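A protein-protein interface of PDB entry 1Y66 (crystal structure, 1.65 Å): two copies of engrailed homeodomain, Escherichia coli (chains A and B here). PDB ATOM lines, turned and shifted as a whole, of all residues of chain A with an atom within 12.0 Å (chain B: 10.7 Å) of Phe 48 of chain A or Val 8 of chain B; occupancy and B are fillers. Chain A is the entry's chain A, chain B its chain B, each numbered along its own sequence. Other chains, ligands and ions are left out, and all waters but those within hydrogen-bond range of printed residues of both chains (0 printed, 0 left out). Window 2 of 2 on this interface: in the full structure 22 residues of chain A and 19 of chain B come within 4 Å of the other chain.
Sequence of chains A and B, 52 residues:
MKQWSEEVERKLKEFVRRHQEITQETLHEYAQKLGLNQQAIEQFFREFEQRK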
ATOM      1  N   GLN A  39      18.265  15.508  14.866  1.00  0.00           N
ATOM      2  CA  GLN A  39      16.992  16.222  15.028  1.00  0.00           C
ATOM      3  C   GLN A  39      17.157  17.633  14.513  1.00  0.00           C
ATOM      4  O   GLN A  39      16.228  18.180  13.902  1.00  0.00           O
ATOM      5  CB  GLN A  39      16.496  16.280  16.482  1.00  0.00           C
ATOM      6  CG  GLN A  39      15.874  15.014  17.042  1.00  0.00           C
ATOM      7  CD  GLN A  39      15.688  15.070  18.573  1.00  0.00           C
ATOM      8  OE1 GLN A  39      15.383  16.134  19.170  1.00  0.00           O
ATOM      9  NE2 GLN A  39      15.849  13.920  19.213  1.00  0.00           N
ATOM     10  N   ALA A  40      18.343  18.201  14.719  1.00  0.00           N
ATOM     11  CA  ALA A  40      18.601  19.599  14.363  1.00  0.00           C
ATOM     12  C   ALA A  40      18.632  19.794  12.825  1.00  0.00           C
ATOM     13  O   ALA A  40      18.133  20.794  12.280  1.00  0.00           O
ATOM     14  CB  ALA A  40      19.931  20.043  14.996  1.00  0.00           C
ATOM     15  N   ILE A  41      19.252  18.862  12.108  1.00  0.00           N
ATOM     16  CA  ILE A  41      19.399  19.046  10.657  1.00  0.00           C
ATOM     17  C   ILE A  41      18.023  18.736  10.039  1.00  0.00           C
ATOM     18  O   ILE A  41      17.652  19.337   9.020  1.00  0.00           O
ATOM     19  CB  ILE A  41      20.562  18.179  10.059  1.00  0.00           C
ATOM     20  CG1 ILE A  41      20.889  18.540   8.601  1.00  0.00           C
ATOM     21  CG2 ILE A  41      20.207  16.706  10.104  1.00  0.00           C
ATOM     22  CD1 ILE A  41      21.170  19.954   8.306  1.00  0.00           C
ATOM     23  N   GLU A  42      17.264  17.820  10.668  1.00  0.00           N
ATOM     24  CA  GLU A  42      15.863  17.570  10.189  1.00  0.00           C
ATOM     25  C   GLU A  42      14.987  18.810  10.325  1.00  0.00           C
ATOM     26  O   GLU A  42      14.206  19.174   9.383  1.00  0.00           O
ATOM     27  CB  GLU A  42      15.222  16.387  10.904  1.00  0.00           C
ATOM     28  CG  GLU A  42      15.804  15.079  10.450  1.00  0.00           C
ATOM     29  CD  GLU A  42      15.284  13.920  11.277  1.00  0.00           C
ATOM     30  OE1 GLU A  42      14.400  14.144  12.156  1.00  0.00           O
ATOM     31  OE2 GLU A  42      15.774  12.792  11.059  1.00  0.00           O
ATOM     32  N   GLN A  43      15.094  19.462  11.479  1.00  0.00           N
ATOM     33  CA  GLN A  43      14.378  20.727  11.744  1.00  0.00           C
ATOM     34  C   GLN A  43      14.769  21.808  10.711  1.00  0.00           C
ATOM     35  O   GLN A  43      13.907  22.518  10.170  1.00  0.00           O
ATOM     36  CB  GLN A  43      14.690  21.241  13.142  1.00  0.00           C
ATOM     37  N   PHE A  44      16.053  21.900  10.392  1.00  0.00           N
ATOM     38  CA  PHE A  44      16.469  22.845   9.358  1.00  0.00           C
ATOM     39  C   PHE A  44      15.820  22.566   8.010  1.00  0.00           C
ATOM     40  O   PHE A  44      15.272  23.484   7.350  1.00  0.00           O
ATOM     41  CB  PHE A  44      17.997  22.858   9.179  1.00  0.00           C
ATOM     42  CG  PHE A  44      18.422  23.541   7.907  1.00  0.00           C
ATOM     43  CD1 PHE A  44      18.342  24.924   7.802  1.00  0.00           C
ATOM     44  CD2 PHE A  44      18.848  22.783   6.808  1.00  0.00           C
ATOM     45  CE1 PHE A  44      18.698  25.576   6.592  1.00  0.00           C
ATOM     46  CE2 PHE A  44      19.199  23.408   5.589  1.00  0.00           C
ATOM     47  CZ  PHE A  44      19.138  24.808   5.490  1.00  0.00           C
ATOM     48  N   PHE A  45      15.814  21.301   7.612  1.00  0.00           N
ATOM     49  CA  PHE A  45      15.191  20.957   6.331  1.00  0.00           C
ATOM     50  C   PHE A  45      13.732  21.399   6.327  1.00  0.00           C
ATOM     51  O   PHE A  45      13.291  22.018   5.361  1.00  0.00           O
ATOM     52  CB  PHE A  45      15.280  19.475   6.015  1.00  0.00           C
ATOM     53  CG  PHE A  45      16.658  19.003   5.615  1.00  0.00           C
ATOM     54  CD1 PHE A  45      17.589  19.862   5.009  1.00  0.00           C
ATOM     55  CD2 PHE A  45      17.010  17.670   5.806  1.00  0.00           C
ATOM     56  CE1 PHE A  45      18.870  19.394   4.621  1.00  0.00           C
ATOM     57  CE2 PHE A  45      18.278  17.196   5.411  1.00  0.00           C
ATOM     58  CZ  PHE A  45      19.199  18.050   4.821  1.00  0.00           C
ATOM     59  N   ARG A  46      12.995  21.112   7.393  1.00  0.00           N
ATOM     60  CA  ARG A  46      11.595  21.561   7.462  1.00  0.00           C
ATOM     61  C   ARG A  46      11.485  23.073   7.364  1.00  0.00           C
ATOM     62  O   ARG A  46      10.685  23.582   6.569  1.00  0.00           O
ATOM     63  CB  ARG A  46      10.901  21.056   8.718  1.00  0.00           C
ATOM     64  CG  ARG A  46      10.768  19.557   8.693  1.00  0.00           C
ATOM     65  CD  ARG A  46      10.024  19.022   9.885  1.00  0.00           C
ATOM     66  NE  ARG A  46      10.761  17.869  10.383  1.00  0.00           N
ATOM     67  CZ  ARG A  46      11.326  17.806  11.579  1.00  0.00           C
ATOM     68  NH1 ARG A  46      11.205  18.815  12.435  1.00  0.00           N
ATOM     69  NH2 ARG A  46      12.008  16.724  11.915  1.00  0.00           N
ATOM     70  N   GLU A  47      12.306  23.787   8.135  1.00  0.00           N
ATOM     71  CA  GLU A  47      12.221  25.251   8.173  1.00  0.00           C
ATOM     72  C   GLU A  47      12.572  25.854   6.845  1.00  0.00           C
ATOM     73  O   GLU A  47      12.002  26.882   6.451  1.00  0.00           O
ATOM     74  CB  GLU A  47      13.122  25.850   9.255  1.00  0.00           C
ATOM     75  CG  GLU A  47      12.659  25.518  10.667  1.00  0.00           C
ATOM     76  CD  GLU A  47      13.612  26.030  11.744  1.00  0.00           C
ATOM     77  OE1 GLU A  47      14.527  26.841  11.412  1.00  0.00           O
ATOM     78  OE2 GLU A  47      13.428  25.624  12.920  1.00  0.00           O
ATOM     79  N   PHE A  48      13.500  25.218   6.148  1.00  0.00           N
ATOM     80  CA  PHE A  48      13.860  25.666   4.836  1.00  0.00           C
ATOM     81  C   PHE A  48      12.703  25.487   3.856  1.00  0.00           C
ATOM     82  O   PHE A  48      12.379  26.419   3.109  1.00  0.00           O
ATOM     83  CB  PHE A  48      15.139  24.988   4.341  1.00  0.00           C
ATOM     84  CG  PHE A  48      15.869  25.800   3.319  1.00  0.00           C
ATOM     85  CD1 PHE A  48      16.465  27.004   3.673  1.00  0.00           C
ATOM     86  CD2 PHE A  48      15.924  25.378   1.998  1.00  0.00           C
ATOM     87  CE1 PHE A  48      17.128  27.764   2.731  1.00  0.00           C
ATOM     88  CE2 PHE A  48      16.581  26.132   1.040  1.00  0.00           C
ATOM     89  CZ  PHE A  48      17.189  27.329   1.406  1.00  0.00           C
ATOM     90  N   GLU A  49      12.066  24.314   3.892  1.00  0.00           N
ATOM     91  CA  GLU A  49      10.911  23.998   3.044  1.00  0.00           C
ATOM     92  C   GLU A  49       9.733  24.950   3.270  1.00  0.00           C
ATOM     93  O   GLU A  49       9.097  25.403   2.302  1.00  0.00           O
ATOM     94  CB  GLU A  49      10.461  22.550   3.270  1.00  0.00           C
ATOM     95  N   GLN A  50       9.447  25.251   4.539  1.00  0.00           N
ATOM     96  CA  GLN A  50       8.375  26.184   4.914  1.00  0.00           C
ATOM     97  C   GLN A  50       8.528  27.511   4.179  1.00  0.00           C
ATOM     98  O   GLN A  50       7.533  28.148   3.831  1.00  0.00           O
ATOM     99  CB  GLN A  50       8.380  26.475   6.420  1.00  0.00           C
ATOM    100  CG  GLN A  50       7.921  25.342   7.352  1.00  0.00           C
ATOM    101  CD  GLN A  50       8.127  25.701   8.834  1.00  0.00           C
ATOM    102  OE1 GLN A  50       7.754  24.939   9.731  1.00  0.00           O
ATOM    103  NE2 GLN A  50       8.732  26.867   9.089  1.00  0.00           N
ATOM    104  N   ARG A  51       9.775  27.921   3.957  1.00  0.00           N
ATOM    105  CA  ARG A  51      10.084  29.218   3.358  1.00  0.00           C
ATOM    106  C   ARG A  51       9.941  29.261   1.826  1.00  0.00           C
ATOM    107  O   ARG A  51      10.002  30.344   1.231  1.00  0.00           O
ATOM    108  CB  ARG A  51      11.489  29.679   3.775  1.00  0.00           C
ATOM    109  CG  ARG A  51      11.635  29.904   5.274  1.00  0.00           C
ATOM    110  CD  ARG A  51      12.802  30.809   5.614  1.00  0.00           C
ATOM    111  NE  ARG A  51      13.948  30.107   6.190  1.00  0.00           N
ATOM    112  CZ  ARG A  51      15.085  29.860   5.543  1.00  0.00           C
ATOM    113  NH1 ARG A  51      15.237  30.235   4.276  1.00  0.00           N
ATOM    114  NH2 ARG A  51      16.075  29.231   6.169  1.00  0.00           N
ATOM    115  N   LYS A  52       9.739  28.100   1.201  1.00  0.00           N
ATOM    116  CA  LYS A  52       9.702  27.996  -0.270  1.00  0.00           C
ATOM    117  C   LYS A  52       8.545  28.772  -0.899  1.00  0.00           C
ATOM    118  O   LYS A  52       7.631  29.229  -0.206  1.00  0.00           O
ATOM    119  CB  LYS A  52       9.648  26.535  -0.716  1.00  0.00           C
ATOM    120  N   SER B   5      20.854  26.786  -2.774  1.00  0.00           N
ATOM    121  CA  SER B   5      21.775  25.681  -3.180  1.00  0.00           C
ATOM    122  C   SER B   5      23.062  25.800  -2.362  1.00  0.00           C
ATOM    123  O   SER B   5      23.509  24.844  -1.708  1.00  0.00           O
ATOM    124  CB  SER B   5      22.072  25.757  -4.691  1.00  0.00           C
ATOM    125  OG  SER B   5      22.890  24.672  -5.128  1.00  0.00           O
ATOM    126  N   GLU B   6      23.638  26.996  -2.382  1.00  0.00           N
ATOM    127  CA  GLU B   6      24.837  27.296  -1.598  1.00  0.00           C
ATOM    128  C   GLU B   6      24.546  27.375  -0.093  1.00  0.00           C
ATOM    129  O   GLU B   6      25.357  26.895   0.714  1.00  0.00           O
ATOM    130  CB  GLU B   6      25.510  28.574  -2.107  1.00  0.00           C
ATOM    131  CG  GLU B   6      26.177  28.419  -3.463  1.00  0.00           C
ATOM    132  N   GLU B   7      23.398  27.944   0.284  1.00  0.00           N
ATOM    133  CA  GLU B   7      23.049  28.109   1.702  1.00  0.00           C
ATOM    134  C   GLU B   7      22.720  26.767   2.366  1.00  0.00           C
ATOM    135  O   GLU B   7      23.061  26.532   3.541  1.00  0.00           O
ATOM    136  CB  GLU B   7      21.903  29.096   1.900  1.00  0.00           C
ATOM    137  N   VAL B   8      22.074  25.878   1.613  1.00  0.00           N
ATOM    138  CA  VAL B   8      21.877  24.521   2.106  1.00  0.00           C
ATOM    139  C   VAL B   8      23.217  23.787   2.243  1.00  0.00           C
ATOM    140  O   VAL B   8      23.481  23.138   3.286  1.00  0.00           O
ATOM    141  CB  VAL B   8      20.894  23.719   1.240  1.00  0.00           C
ATOM    142  CG1 VAL B   8      20.700  22.362   1.848  1.00  0.00           C
ATOM    143  CG2 VAL B   8      19.579  24.441   1.194  1.00  0.00           C
ATOM    144  N   GLU B   9      24.077  23.919   1.231  1.00  0.00           N
ATOM    145  CA  GLU B   9      25.379  23.260   1.288  1.00  0.00           C
ATOM    146  C   GLU B   9      26.164  23.751   2.506  1.00  0.00           C
ATOM    147  O   GLU B   9      26.844  22.962   3.172  1.00  0.00           O
ATOM    148  CB  GLU B   9      26.177  23.472   0.021  1.00  0.00           C
ATOM    149  N   ARG B  10      26.066  25.038   2.828  1.00  0.00           N
ATOM    150  CA  ARG B  10      26.794  25.527   4.015  1.00  0.00           C
ATOM    151  C   ARG B  10      26.203  24.974   5.324  1.00  0.00           C
ATOM    152  O   ARG B  10      26.928  24.677   6.277  1.00  0.00           O
ATOM    153  CB  ARG B  10      26.942  27.064   4.035  1.00  0.00           C
ATOM    154  CG  ARG B  10      28.047  27.575   3.058  1.00  0.00           C
ATOM    155  CD  ARG B  10      28.291  29.116   3.153  1.00  0.00           C
ATOM    156  NE  ARG B  10      27.057  29.830   2.829  1.00  0.00           N
ATOM    157  CZ  ARG B  10      26.752  30.320   1.623  1.00  0.00           C
ATOM    158  NH1 ARG B  10      27.612  30.239   0.596  1.00  0.00           N
ATOM    159  NH2 ARG B  10      25.576  30.911   1.459  1.00  0.00           N
ATOM    160  N   LYS B  11      24.881  24.803   5.378  1.00  0.00           N
ATOM    161  CA  LYS B  11      24.265  24.311   6.618  1.00  0.00           C
ATOM    162  C   LYS B  11      24.646  22.829   6.816  1.00  0.00           C
ATOM    163  O   LYS B  11      24.842  22.361   7.944  1.00  0.00           O
ATOM    164  CB  LYS B  11      22.732  24.467   6.590  1.00  0.00           C
ATOM    165  CG  LYS B  11      22.110  24.339   7.953  1.00  0.00           C
ATOM    166  CD  LYS B  11      21.968  25.694   8.648  1.00  0.00           C
ATOM    167  N   LEU B  12      24.750  22.101   5.715  1.00  0.00           N
ATOM    168  CA  LEU B  12      25.202  20.714   5.756  1.00  0.00           C
ATOM    169  C   LEU B  12      26.657  20.644   6.199  1.00  0.00           C
ATOM    170  O   LEU B  12      27.075  19.691   6.869  1.00  0.00           O
ATOM    171  CB  LEU B  12      25.035  20.041   4.388  1.00  0.00           C
ATOM    172  CG  LEU B  12      23.716  19.236   4.267  1.00  0.00           C
ATOM    173  CD1 LEU B  12      23.288  18.573   5.568  1.00  0.00           C
ATOM    174  CD2 LEU B  12      22.601  20.104   3.802  1.00  0.00           C
ATOM    175  N   LYS B  13      27.441  21.638   5.775  1.00  0.00           N
ATOM    176  CA  LYS B  13      28.822  21.718   6.262  1.00  0.00           C
ATOM    177  C   LYS B  13      28.866  21.795   7.774  1.00  0.00           C
ATOM    178  O   LYS B  13      29.707  21.110   8.418  1.00  0.00           O
ATOM    179  CB  LYS B  13      29.576  22.920   5.617  1.00  0.00           C
ATOM    180  CG  LYS B  13      29.973  22.630   4.209  1.00  0.00           C
ATOM    181  CD  LYS B  13      31.188  21.679   4.186  1.00  0.00           C
ATOM    182  CE  LYS B  13      32.509  22.404   4.343  1.00  0.00           C
ATOM    183  NZ  LYS B  13      33.636  21.546   3.809  1.00  0.00           N
ATOM    184  N   GLU B  14      28.007  22.611   8.358  1.00  0.00           N
ATOM    185  CA  GLU B  14      28.031  22.750   9.799  1.00  0.00           C
ATOM    186  C   GLU B  14      27.535  21.435  10.459  1.00  0.00           C
ATOM    187  O   GLU B  14      28.025  21.038  11.513  1.00  0.00           O
ATOM    188  CB  GLU B  14      27.211  23.970  10.248  1.00  0.00           C
ATOM    189  CG  GLU B  14      27.043  24.128  11.792  1.00  0.00           C
ATOM    190  CD  GLU B  14      28.376  24.175  12.647  1.00  0.00           C
ATOM    191  OE1 GLU B  14      29.483  24.337  12.097  1.00  0.00           O
ATOM    192  OE2 GLU B  14      28.287  24.063  13.894  1.00  0.00           O
ATOM    193  N   PHE B  15      26.573  20.753   9.843  1.00  0.00           N
ATOM    194  CA  PHE B  15      26.148  19.448  10.406  1.00  0.00           C
ATOM    195  C   PHE B  15      27.260  18.429  10.418  1.00  0.00           C
ATOM    196  O   PHE B  15      27.474  17.719  11.393  1.00  0.00           O
ATOM    197  CB  PHE B  15      24.846  18.990   9.742  1.00  0.00           C
ATOM    198  CG  PHE B  15      24.643  17.427   9.757  1.00  0.00           C
ATOM    199  CD1 PHE B  15      24.006  16.826  10.846  1.00  0.00           C
ATOM    200  CD2 PHE B  15      25.104  16.575   8.706  1.00  0.00           C
ATOM    201  CE1 PHE B  15      23.808  15.423  10.895  1.00  0.00           C
ATOM    202  CE2 PHE B  15      24.927  15.167   8.741  1.00  0.00           C
ATOM    203  CZ  PHE B  15      24.267  14.601   9.870  1.00  0.00           C
ATOM    204  N   VAL B  16      27.977  18.360   9.312  1.00  0.00           N
ATOM    205  CA  VAL B  16      29.105  17.437   9.250  1.00  0.00           C
ATOM    206  C   VAL B  16      30.191  17.817  10.264  1.00  0.00           C
ATOM    207  O   VAL B  16      30.777  16.936  10.929  1.00  0.00           O
ATOM    208  CB  VAL B  16      29.640  17.405   7.827  1.00  0.00           C
ATOM    209  CG1 VAL B  16      30.997  16.723   7.771  1.00  0.00           C
ATOM    210  CG2 VAL B  16      28.563  16.779   6.902  1.00  0.00           C
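No position is printed for both chains.
Of the 5 pairs that touch across the chains among the printed residues, none has its exchanged pair printed and touching as well.
Among the printed residues, pairs that only touch across the chains: Phe 48 of chain A with Val 8 of chain B (3.4 Å), Ile 41 of chain A with Leu 12 of chain B (3.7 Å), Phe 44 of chain A with Lys 11 of chain B (3.8 Å), Ile 41 of chain A with Phe 15 of chain B (3.8 Å) and Phe 45 of chain A with Leu 12 of chain B (3.9 Å).
Of the 14 printed residues of chain A, 4 touch a printed residue of chain B.
Hydrophobic or aromatic side chains of chain A that line the printed part of chain B: Ile 41, Phe 44, Phe 45 and Phe 48.
Among the printed residues, 5 pairs touch across the chains.
Phe 48 of chain A touches one residue of chain B.
Val 8 of chain B touches just one residue of chain A: Phe 48.
Of the printed residues of chain B, Phe 44 of chain A touches Lys 11.
No residue of chain B comes within 4 Å of Glu 49 of chain A.
No residue of chain B comes within 4 Å of Arg 51 of chain A.
No residue of chain B comes within 4 Å of Lys 52 of chain A.
No residue of chain A comes within 4 Å of Glu 6 of chain B.
No residue of chain A comes within 4 Å of Glu 9 of chain B.
No residue of chain A comes within 4 Å of Arg 10 of chain B.
Leu 12 of chain B touches two residues of chain A.
Of the printed residues of chain B, Ile 41 of chain A touches Leu 12 and Phe 15.
Of the printed residues of chain B, Phe 45 of chain A touches Leu 12 (3.9 Å).
Of the printed residues of chain A, Phe 15 of chain B touches Ile 41 (3.8 Å).
Gln 43 of chain A touches none of the printed residues of chain B.
Glu 47 of chain A touches none of the printed residues of chain B.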
